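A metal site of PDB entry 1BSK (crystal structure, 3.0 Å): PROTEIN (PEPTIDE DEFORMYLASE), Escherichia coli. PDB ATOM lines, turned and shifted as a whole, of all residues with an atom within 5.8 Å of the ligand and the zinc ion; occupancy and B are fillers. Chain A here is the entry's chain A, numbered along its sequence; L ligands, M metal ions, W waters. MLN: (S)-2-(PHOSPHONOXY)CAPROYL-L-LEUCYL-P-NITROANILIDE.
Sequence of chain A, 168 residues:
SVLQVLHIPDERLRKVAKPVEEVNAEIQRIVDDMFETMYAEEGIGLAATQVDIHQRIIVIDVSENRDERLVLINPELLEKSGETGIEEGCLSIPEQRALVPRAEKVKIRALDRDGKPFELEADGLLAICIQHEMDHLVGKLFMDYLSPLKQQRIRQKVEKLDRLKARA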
ATOM      1  N   GLU A  41      25.780   7.611  21.702  1.00  0.00           N
ATOM      2  CA  GLU A  41      25.292   8.810  21.034  1.00  0.00           C
ATOM      3  C   GLU A  41      24.644   9.825  21.954  1.00  0.00           C
ATOM      4  O   GLU A  41      24.190  10.867  21.502  1.00  0.00           O
ATOM      5  CB  GLU A  41      24.318   8.399  19.956  1.00  0.00           C
ATOM      6  CG  GLU A  41      24.805   7.233  19.135  1.00  0.00           C
ATOM      7  CD  GLU A  41      25.645   7.671  17.974  1.00  0.00           C
ATOM      8  OE1 GLU A  41      26.798   8.077  18.218  1.00  0.00           O
ATOM      9  OE2 GLU A  41      25.129   7.588  16.829  1.00  0.00           O
ATOM     10  N   GLU A  42      24.599   9.525  23.255  1.00  0.00           N
ATOM     11  CA  GLU A  42      23.979  10.443  24.216  1.00  0.00           C
ATOM     12  C   GLU A  42      22.494  10.682  23.977  1.00  0.00           C
ATOM     13  O   GLU A  42      21.962  11.774  24.247  1.00  0.00           O
ATOM     14  CB  GLU A  42      24.722  11.782  24.279  1.00  0.00           C
ATOM     15  CG  GLU A  42      26.211  11.672  24.668  1.00  0.00           C
ATOM     16  CD  GLU A  42      26.851  13.034  24.953  1.00  0.00           C
ATOM     17  OE1 GLU A  42      27.351  13.688  23.996  1.00  0.00           O
ATOM     18  OE2 GLU A  42      26.890  13.411  26.137  1.00  0.00           O
ATOM     19  N   GLY A  43      21.817   9.671  23.427  1.00  0.00           N
ATOM     20  CA  GLY A  43      20.392   9.788  23.189  1.00  0.00           C
ATOM     21  C   GLY A  43      19.669   9.327  24.415  1.00  0.00           C
ATOM     22  O   GLY A  43      20.248   8.602  25.226  1.00  0.00           O
ATOM     23  N   ILE A  44      18.418   9.757  24.581  1.00  0.00           N
ATOM     24  CA  ILE A  44      17.610   9.333  25.738  1.00  0.00           C
ATOM     25  C   ILE A  44      16.695   8.142  25.417  1.00  0.00           C
ATOM     26  O   ILE A  44      16.000   7.610  26.281  1.00  0.00           O
ATOM     27  CB  ILE A  44      16.814  10.523  26.400  1.00  0.00           C
ATOM     28  CG1 ILE A  44      15.642  10.979  25.516  1.00  0.00           C
ATOM     29  CG2 ILE A  44      17.693  11.712  26.619  1.00  0.00           C
ATOM     30  CD1 ILE A  44      14.823  12.141  26.103  1.00  0.00           C
ATOM     31  N   GLY A  45      16.695   7.715  24.166  1.00  0.00           N
ATOM     32  CA  GLY A  45      15.883   6.592  23.755  1.00  0.00           C
ATOM     33  C   GLY A  45      16.376   6.092  22.404  1.00  0.00           C
ATOM     34  O   GLY A  45      17.258   6.710  21.793  1.00  0.00           O
ATOM     35  N   LEU A  46      15.841   4.969  21.953  1.00  0.00           N
ATOM     36  CA  LEU A  46      16.228   4.410  20.645  1.00  0.00           C
ATOM     37  C   LEU A  46      15.286   3.318  20.167  1.00  0.00           C
ATOM     38  O   LEU A  46      15.063   2.323  20.862  1.00  0.00           O
ATOM     39  CB  LEU A  46      17.658   3.836  20.708  1.00  0.00           C
ATOM     40  CG  LEU A  46      18.193   3.377  19.345  1.00  0.00           C
ATOM     41  CD1 LEU A  46      18.688   4.573  18.555  1.00  0.00           C
ATOM     42  CD2 LEU A  46      19.332   2.421  19.529  1.00  0.00           C
ATOM     43  N   ALA A  47      14.699   3.519  19.005  1.00  0.00           N
ATOM     44  CA  ALA A  47      13.796   2.522  18.422  1.00  0.00           C
ATOM     45  C   ALA A  47      14.590   1.597  17.483  1.00  0.00           C
ATOM     46  O   ALA A  47      15.477   2.055  16.761  1.00  0.00           O
ATOM     47  CB  ALA A  47      12.689   3.169  17.688  1.00  0.00           C
ATOM     48  N   GLN A  50      15.548   2.519  13.862  1.00  0.00           N
ATOM     49  CA  GLN A  50      16.656   3.423  13.587  1.00  0.00           C
ATOM     50  C   GLN A  50      17.951   2.693  13.274  1.00  0.00           C
ATOM     51  O   GLN A  50      18.764   3.199  12.517  1.00  0.00           O
ATOM     52  CB  GLN A  50      16.885   4.352  14.775  1.00  0.00           C
ATOM     53  CG  GLN A  50      15.743   5.298  15.069  1.00  0.00           C
ATOM     54  CD  GLN A  50      16.006   6.091  16.331  1.00  0.00           C
ATOM     55  OE1 GLN A  50      15.595   5.704  17.409  1.00  0.00           O
ATOM     56  NE2 GLN A  50      16.700   7.213  16.196  1.00  0.00           N
ATOM     57  N   ILE A  86       8.090  19.625  23.518  1.00  0.00           N
ATOM     58  CA  ILE A  86       9.471  20.014  23.761  1.00  0.00           C
ATOM     59  C   ILE A  86      10.251  20.081  22.439  1.00  0.00           C
ATOM     60  O   ILE A  86       9.781  19.582  21.403  1.00  0.00           O
ATOM     61  CB  ILE A  86      10.203  19.014  24.688  1.00  0.00           C
ATOM     62  CG1 ILE A  86      10.316  17.653  24.005  1.00  0.00           C
ATOM     63  CG2 ILE A  86       9.468  18.824  26.004  1.00  0.00           C
ATOM     64  CD1 ILE A  86      11.215  16.687  24.716  1.00  0.00           C
ATOM     65  N   GLU A  87      11.405  20.742  22.454  1.00  0.00           N
ATOM     66  CA  GLU A  87      12.242  20.844  21.267  1.00  0.00           C
ATOM     67  C   GLU A  87      12.900  19.482  21.087  1.00  0.00           C
ATOM     68  O   GLU A  87      14.024  19.250  21.560  1.00  0.00           O
ATOM     69  CB  GLU A  87      13.280  21.928  21.452  1.00  0.00           C
ATOM     70  CG  GLU A  87      12.671  23.230  21.905  1.00  0.00           C
ATOM     71  CD  GLU A  87      12.659  24.262  20.818  1.00  0.00           C
ATOM     72  OE1 GLU A  87      11.930  24.042  19.842  1.00  0.00           O
ATOM     73  OE2 GLU A  87      13.347  25.290  20.965  1.00  0.00           O
ATOM     74  N   GLU A  88      12.204  18.599  20.389  1.00  0.00           N
ATOM     75  CA  GLU A  88      12.695  17.263  20.156  1.00  0.00           C
ATOM     76  C   GLU A  88      13.806  17.186  19.146  1.00  0.00           C
ATOM     77  O   GLU A  88      13.873  17.997  18.222  1.00  0.00           O
ATOM     78  CB  GLU A  88      11.568  16.335  19.738  1.00  0.00           C
ATOM     79  CG  GLU A  88      10.585  16.051  20.854  1.00  0.00           C
ATOM     80  CD  GLU A  88       9.455  15.158  20.427  1.00  0.00           C
ATOM     81  OE1 GLU A  88       9.681  14.311  19.558  1.00  0.00           O
ATOM     82  OE2 GLU A  88       8.333  15.297  20.971  1.00  0.00           O
ATOM     83  N   GLY A  89      14.656  16.182  19.314  1.00  0.00           N
ATOM     84  CA  GLY A  89      15.748  15.931  18.412  1.00  0.00           C
ATOM     85  C   GLY A  89      15.689  14.464  18.085  1.00  0.00           C
ATOM     86  O   GLY A  89      14.909  13.739  18.703  1.00  0.00           O
ATOM     87  N   CYS A  90      16.495  14.020  17.129  1.00  0.00           N
ATOM     88  CA  CYS A  90      16.509  12.613  16.762  1.00  0.00           C
ATOM     89  C   CYS A  90      17.896  12.312  16.193  1.00  0.00           C
ATOM     90  O   CYS A  90      18.488  13.157  15.535  1.00  0.00           O
ATOM     91  CB  CYS A  90      15.419  12.330  15.748  1.00  0.00           C
ATOM     92  SG  CYS A  90      15.218  10.575  15.349  1.00  0.00           S
ATOM     93  N   LEU A  91      18.416  11.123  16.456  1.00  0.00           N
ATOM     94  CA  LEU A  91      19.711  10.750  15.939  1.00  0.00           C
ATOM     95  C   LEU A  91      19.624  10.464  14.439  1.00  0.00           C
ATOM     96  O   LEU A  91      20.653  10.355  13.750  1.00  0.00           O
ATOM     97  CB  LEU A  91      20.221   9.507  16.672  1.00  0.00           C
ATOM     98  CG  LEU A  91      20.618   9.679  18.141  1.00  0.00           C
ATOM     99  CD1 LEU A  91      21.047   8.334  18.684  1.00  0.00           C
ATOM    100  CD2 LEU A  91      21.749  10.702  18.293  1.00  0.00           C
ATOM    101  N   SER A  92      18.389  10.332  13.939  1.00  0.00           N
ATOM    102  CA  SER A  92      18.110  10.092  12.522  1.00  0.00           C
ATOM    103  C   SER A  92      17.914  11.400  11.765  1.00  0.00           C
ATOM    104  O   SER A  92      17.918  11.438  10.544  1.00  0.00           O
ATOM    105  CB  SER A  92      16.880   9.175  12.344  1.00  0.00           C
ATOM    106  OG  SER A  92      17.155   7.823  12.723  1.00  0.00           O
ATOM    107  N   ARG A  97      15.858  20.357  15.425  1.00  0.00           N
ATOM    108  CA  ARG A  97      14.997  20.298  16.606  1.00  0.00           C
ATOM    109  C   ARG A  97      13.711  21.033  16.313  1.00  0.00           C
ATOM    110  O   ARG A  97      13.737  22.138  15.765  1.00  0.00           O
ATOM    111  CB  ARG A  97      15.655  21.002  17.802  1.00  0.00           C
ATOM    112  CG  ARG A  97      16.989  20.460  18.254  1.00  0.00           C
ATOM    113  CD  ARG A  97      16.879  19.603  19.511  1.00  0.00           C
ATOM    114  NE  ARG A  97      18.150  18.924  19.791  1.00  0.00           N
ATOM    115  CZ  ARG A  97      18.654  18.736  21.007  1.00  0.00           C
ATOM    116  NH1 ARG A  97      18.023  19.197  22.082  1.00  0.00           N
ATOM    117  NH2 ARG A  97      19.858  18.172  21.136  1.00  0.00           N
ATOM    118  N   LEU A 125       8.858  14.025  30.572  1.00  0.00           N
ATOM    119  CA  LEU A 125       9.764  13.653  29.502  1.00  0.00           C
ATOM    120  C   LEU A 125       9.637  12.193  29.156  1.00  0.00           C
ATOM    121  O   LEU A 125       9.674  11.853  27.999  1.00  0.00           O
ATOM    122  CB  LEU A 125      11.195  13.976  29.878  1.00  0.00           C
ATOM    123  CG  LEU A 125      12.298  13.802  28.824  1.00  0.00           C
ATOM    124  CD1 LEU A 125      12.167  14.897  27.784  1.00  0.00           C
ATOM    125  CD2 LEU A 125      13.667  13.857  29.506  1.00  0.00           C
ATOM    126  N   ILE A 128       6.816  11.774  26.783  1.00  0.00           N
ATOM    127  CA  ILE A 128       7.122  12.303  25.465  1.00  0.00           C
ATOM    128  C   ILE A 128       8.042  11.329  24.712  1.00  0.00           C
ATOM    129  O   ILE A 128       7.718  10.906  23.600  1.00  0.00           O
ATOM    130  CB  ILE A 128       7.757  13.701  25.537  1.00  0.00           C
ATOM    131  CG1 ILE A 128       6.721  14.688  26.127  1.00  0.00           C
ATOM    132  CG2 ILE A 128       8.185  14.163  24.138  1.00  0.00           C
ATOM    133  CD1 ILE A 128       7.246  16.069  26.371  1.00  0.00           C
ATOM    134  N   CYS A 129       9.122  10.908  25.351  1.00  0.00           N
ATOM    135  CA  CYS A 129      10.083   9.952  24.786  1.00  0.00           C
ATOM    136  C   CYS A 129       9.368   8.711  24.197  1.00  0.00           C
ATOM    137  O   CYS A 129       9.571   8.396  23.023  1.00  0.00           O
ATOM    138  CB  CYS A 129      11.091   9.531  25.861  1.00  0.00           C
ATOM    139  SG  CYS A 129      12.518   8.661  25.213  1.00  0.00           S
ATOM    140  N   HIS A 132       7.556   9.366  21.098  1.00  0.00           N
ATOM    141  CA  HIS A 132       8.555   9.562  20.039  1.00  0.00           C
ATOM    142  C   HIS A 132       9.051   8.219  19.516  1.00  0.00           C
ATOM    143  O   HIS A 132       8.995   7.975  18.306  1.00  0.00           O
ATOM    144  CB  HIS A 132       9.769  10.403  20.520  1.00  0.00           C
ATOM    145  CG  HIS A 132      10.812  10.650  19.471  1.00  0.00           C
ATOM    146  ND1 HIS A 132      11.077  11.893  18.918  1.00  0.00           N
ATOM    147  CD2 HIS A 132      11.689   9.800  18.887  1.00  0.00           C
ATOM    148  CE1 HIS A 132      12.069  11.760  18.048  1.00  0.00           C
ATOM    149  NE2 HIS A 132      12.482  10.505  17.993  1.00  0.00           N
ATOM    150  N   GLU A 133       9.527   7.384  20.421  1.00  0.00           N
ATOM    151  CA  GLU A 133      10.054   6.045  20.093  1.00  0.00           C
ATOM    152  C   GLU A 133       9.040   5.075  19.474  1.00  0.00           C
ATOM    153  O   GLU A 133       9.429   4.210  18.668  1.00  0.00           O
ATOM    154  CB  GLU A 133      10.711   5.417  21.326  1.00  0.00           C
ATOM    155  CG  GLU A 133      11.873   6.215  21.882  1.00  0.00           C
ATOM    156  CD  GLU A 133      12.904   6.612  20.835  1.00  0.00           C
ATOM    157  OE1 GLU A 133      13.072   5.875  19.851  1.00  0.00           O
ATOM    158  OE2 GLU A 133      13.546   7.660  21.041  1.00  0.00           O
ATOM    159  N   HIS A 136       8.495   5.883  15.787  1.00  0.00           N
ATOM    160  CA  HIS A 136       9.611   5.294  15.066  1.00  0.00           C
ATOM    161  C   HIS A 136       9.292   3.877  14.623  1.00  0.00           C
ATOM    162  O   HIS A 136       9.738   3.442  13.564  1.00  0.00           O
ATOM    163  CB  HIS A 136      10.847   5.242  15.951  1.00  0.00           C
ATOM    164  CG  HIS A 136      11.805   6.361  15.752  1.00  0.00           C
ATOM    165  ND1 HIS A 136      12.178   6.811  14.501  1.00  0.00           N
ATOM    166  CD2 HIS A 136      12.481   7.108  16.654  1.00  0.00           C
ATOM    167  CE1 HIS A 136      13.054   7.777  14.700  1.00  0.00           C
ATOM    168  NE2 HIS A 136      13.258   7.985  15.991  1.00  0.00           N
ATOM    169  N   LEU A 141       8.372   9.805  11.815  1.00  0.00           N
ATOM    170  CA  LEU A 141       9.458  10.608  12.399  1.00  0.00           C
ATOM    171  C   LEU A 141       8.834  11.889  12.928  1.00  0.00           C
ATOM    172  O   LEU A 141       7.742  12.262  12.514  1.00  0.00           O
ATOM    173  CB  LEU A 141      10.523  10.931  11.339  1.00  0.00           C
ATOM    174  CG  LEU A 141      11.256   9.717  10.790  1.00  0.00           C
ATOM    175  CD1 LEU A 141      11.964  10.009   9.497  1.00  0.00           C
ATOM    176  CD2 LEU A 141      12.248   9.227  11.807  1.00  0.00           C
ATOM    177  N   PHE A 142       9.539  12.585  13.826  1.00  0.00           N
ATOM    178  CA  PHE A 142       8.976  13.800  14.407  1.00  0.00           C
ATOM    179  C   PHE A 142       8.693  14.916  13.422  1.00  0.00           C
ATOM    180  O   PHE A 142       7.844  15.778  13.692  1.00  0.00           O
ATOM    181  CB  PHE A 142       9.826  14.309  15.599  1.00  0.00           C
ATOM    182  CG  PHE A 142      11.009  15.143  15.204  1.00  0.00           C
ATOM    183  CD1 PHE A 142      10.859  16.474  14.844  1.00  0.00           C
ATOM    184  CD2 PHE A 142      12.283  14.603  15.231  1.00  0.00           C
ATOM    185  CE1 PHE A 142      11.966  17.267  14.522  1.00  0.00           C
ATOM    186  CE2 PHE A 142      13.395  15.387  14.899  1.00  0.00           C
ATOM    187  CZ  PHE A 142      13.227  16.720  14.550  1.00  0.00           C
HETATM  188  O3  MLN L   1      14.913   8.526  18.574  1.00  0.00           O
HETATM  189  P1  MLN L   1      16.343   8.671  19.312  1.00  0.00           P
HETATM  190  O2  MLN L   1      16.079   9.560  20.831  1.00  0.00           O
HETATM  191  O4  MLN L   1      17.397   9.283  18.298  1.00  0.00           O
HETATM  192  C5  MLN L   1      15.787  10.914  20.684  1.00  0.00           C
HETATM  193  C6  MLN L   1      16.872  11.652  21.414  1.00  0.00           C
HETATM  194  C7  MLN L   1      14.332  10.847  21.259  1.00  0.00           C
HETATM  195  C8  MLN L   1      13.938  11.385  22.656  1.00  0.00           C
HETATM  196  C9  MLN L   1      12.607  12.169  22.861  1.00  0.00           C
HETATM  197  C10 MLN L   1      12.769  13.397  21.992  1.00  0.00           C
HETATM  198  O11 MLN L   1      17.657  11.101  22.138  1.00  0.00           O
HETATM  199  N12 MLN L   1      16.845  12.991  21.146  1.00  0.00           N
HETATM  200  C13 MLN L   1      17.713  13.927  21.837  1.00  0.00           C
HETATM  201  C14 MLN L   1      18.615  14.537  20.781  1.00  0.00           C
HETATM  202  C15 MLN L   1      19.550  13.466  20.265  1.00  0.00           C
HETATM  203  C16 MLN L   1      20.266  14.009  19.077  1.00  0.00           C
HETATM  204  C17 MLN L   1      20.637  13.041  21.237  1.00  0.00           C
HETATM  205  C18 MLN L   1      16.688  14.803  22.521  1.00  0.00           C
HETATM  206  N19 MLN L   1      16.853  15.052  24.020  1.00  0.00           N
HETATM  207  O20 MLN L   1      15.759  15.273  21.896  1.00  0.00           O
HETATM  208  C21 MLN L   1      16.144  15.870  24.738  1.00  0.00           C
HETATM  209  C22 MLN L   1      15.298  16.864  24.174  1.00  0.00           C
HETATM  210  C23 MLN L   1      14.716  17.808  25.037  1.00  0.00           C
HETATM  211  C24 MLN L   1      14.878  17.638  26.460  1.00  0.00           C
HETATM  212  C25 MLN L   1      15.691  16.631  27.028  1.00  0.00           C
HETATM  213  C26 MLN L   1      16.283  15.685  26.143  1.00  0.00           C
HETATM  214  N27 MLN L   1      14.180  18.528  27.330  1.00  0.00           N
HETATM  215  O28 MLN L   1      14.161  18.369  28.619  1.00  0.00           O
HETATM  216  O29 MLN L   1      13.519  19.540  26.763  1.00  0.00           O
HETATM  217 ZN    ZN M   1      14.059   9.576  17.049  1.00  0.00          ZN
HETATM  218  O   HOH W   1      12.072  11.347  15.037  1.00  0.00           O
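The zinc ion is bound by an oxygen (O3) of the ligand, a ring nitrogen (NE2) of His 132, a ring nitrogen (NE2) of His 136 and the side-chain sulfur of Cys 90.
O of Gly 45 lies close to O2 of the ligand (3.2 Å). Glu 42 touches the ligand. Gly 43 touches the ligand (CA to O11, 3.2 Å). CD1 of Ile 86 touches C23 of the ligand, at 3.7 Å. Glu 87 touches the ligand. CG of Glu 88 touches C10 of the ligand, 3.6 Å away. NH2 of Arg 97 touches C14 of the ligand, 3.9 Å away. Leu 125 touches the ligand (CD1 to C25, 3.9996 Å). Cys 129 touches the ligand (CA to C9, 3.9 Å). Hydrophobic or aromatic side chains within 4 Å of the ligand: Ile 44, Ile 86, Leu 91, Leu 125, His 132 and His 136. The nearest printed residue that does not touch the ligand is Glu 41 (4.2 Å).
Merely in contact with the zinc ion: Gln 50 (3.6 Å). Within 4 Å of the zinc ion: Gln 50, Cys 90, His 132 and His 136. Along chain A the residues within 4 Å of the zinc ion span positions 50 to 136. The nearest printed residue that does not touch the zinc ion is Glu 133 (4.5 Å).
A ring nitrogen (ND1) of His 132 sits at hydrogen-bond distance from the side-chain carboxylate (OE1) of Glu 88, 2.9 Å away. The backbone carbonyl oxygen (O) of Ile 44 lies within hydrogen-bond range of the side-chain sulfur (SG) of Cys 129 (3.8 Å). OE1 of Gln 50 is in hydrogen-bond range of N of Ala 47 (2.9 Å). SG of Cys 90 lies close to N of Ser 92, at 3.5 Å. The side-chain sulfur of Cys 90 sits close to the side-chain amide nitrogen of Gln 50, 3.8 Å away. The side-chain carboxylate (OE1) of Glu 133 is in hydrogen-bond range of the backbone NH (N) of Ala 47 (3.0 Å).
A nitrogen (N12) of the ligand is in hydrogen-bond range of the backbone carbonyl oxygen of Gly 89, at 3.2 Å. OE2 of Glu 133 lies close to O3 of the ligand (3.0 Å). The backbone NH of Leu 91 is in hydrogen-bond range of an oxygen (O4) of the ligand. The side-chain amide nitrogen of Gln 50 is in hydrogen-bond range of an oxygen (O4) of the ligand (3.0 Å). N of Gly 89 is in hydrogen-bond range of O20 of the ligand (3.0 Å). The backbone NH (N) of Ile 44 is in hydrogen-bond range of an oxygen (O11) of the ligand (2.9 Å).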
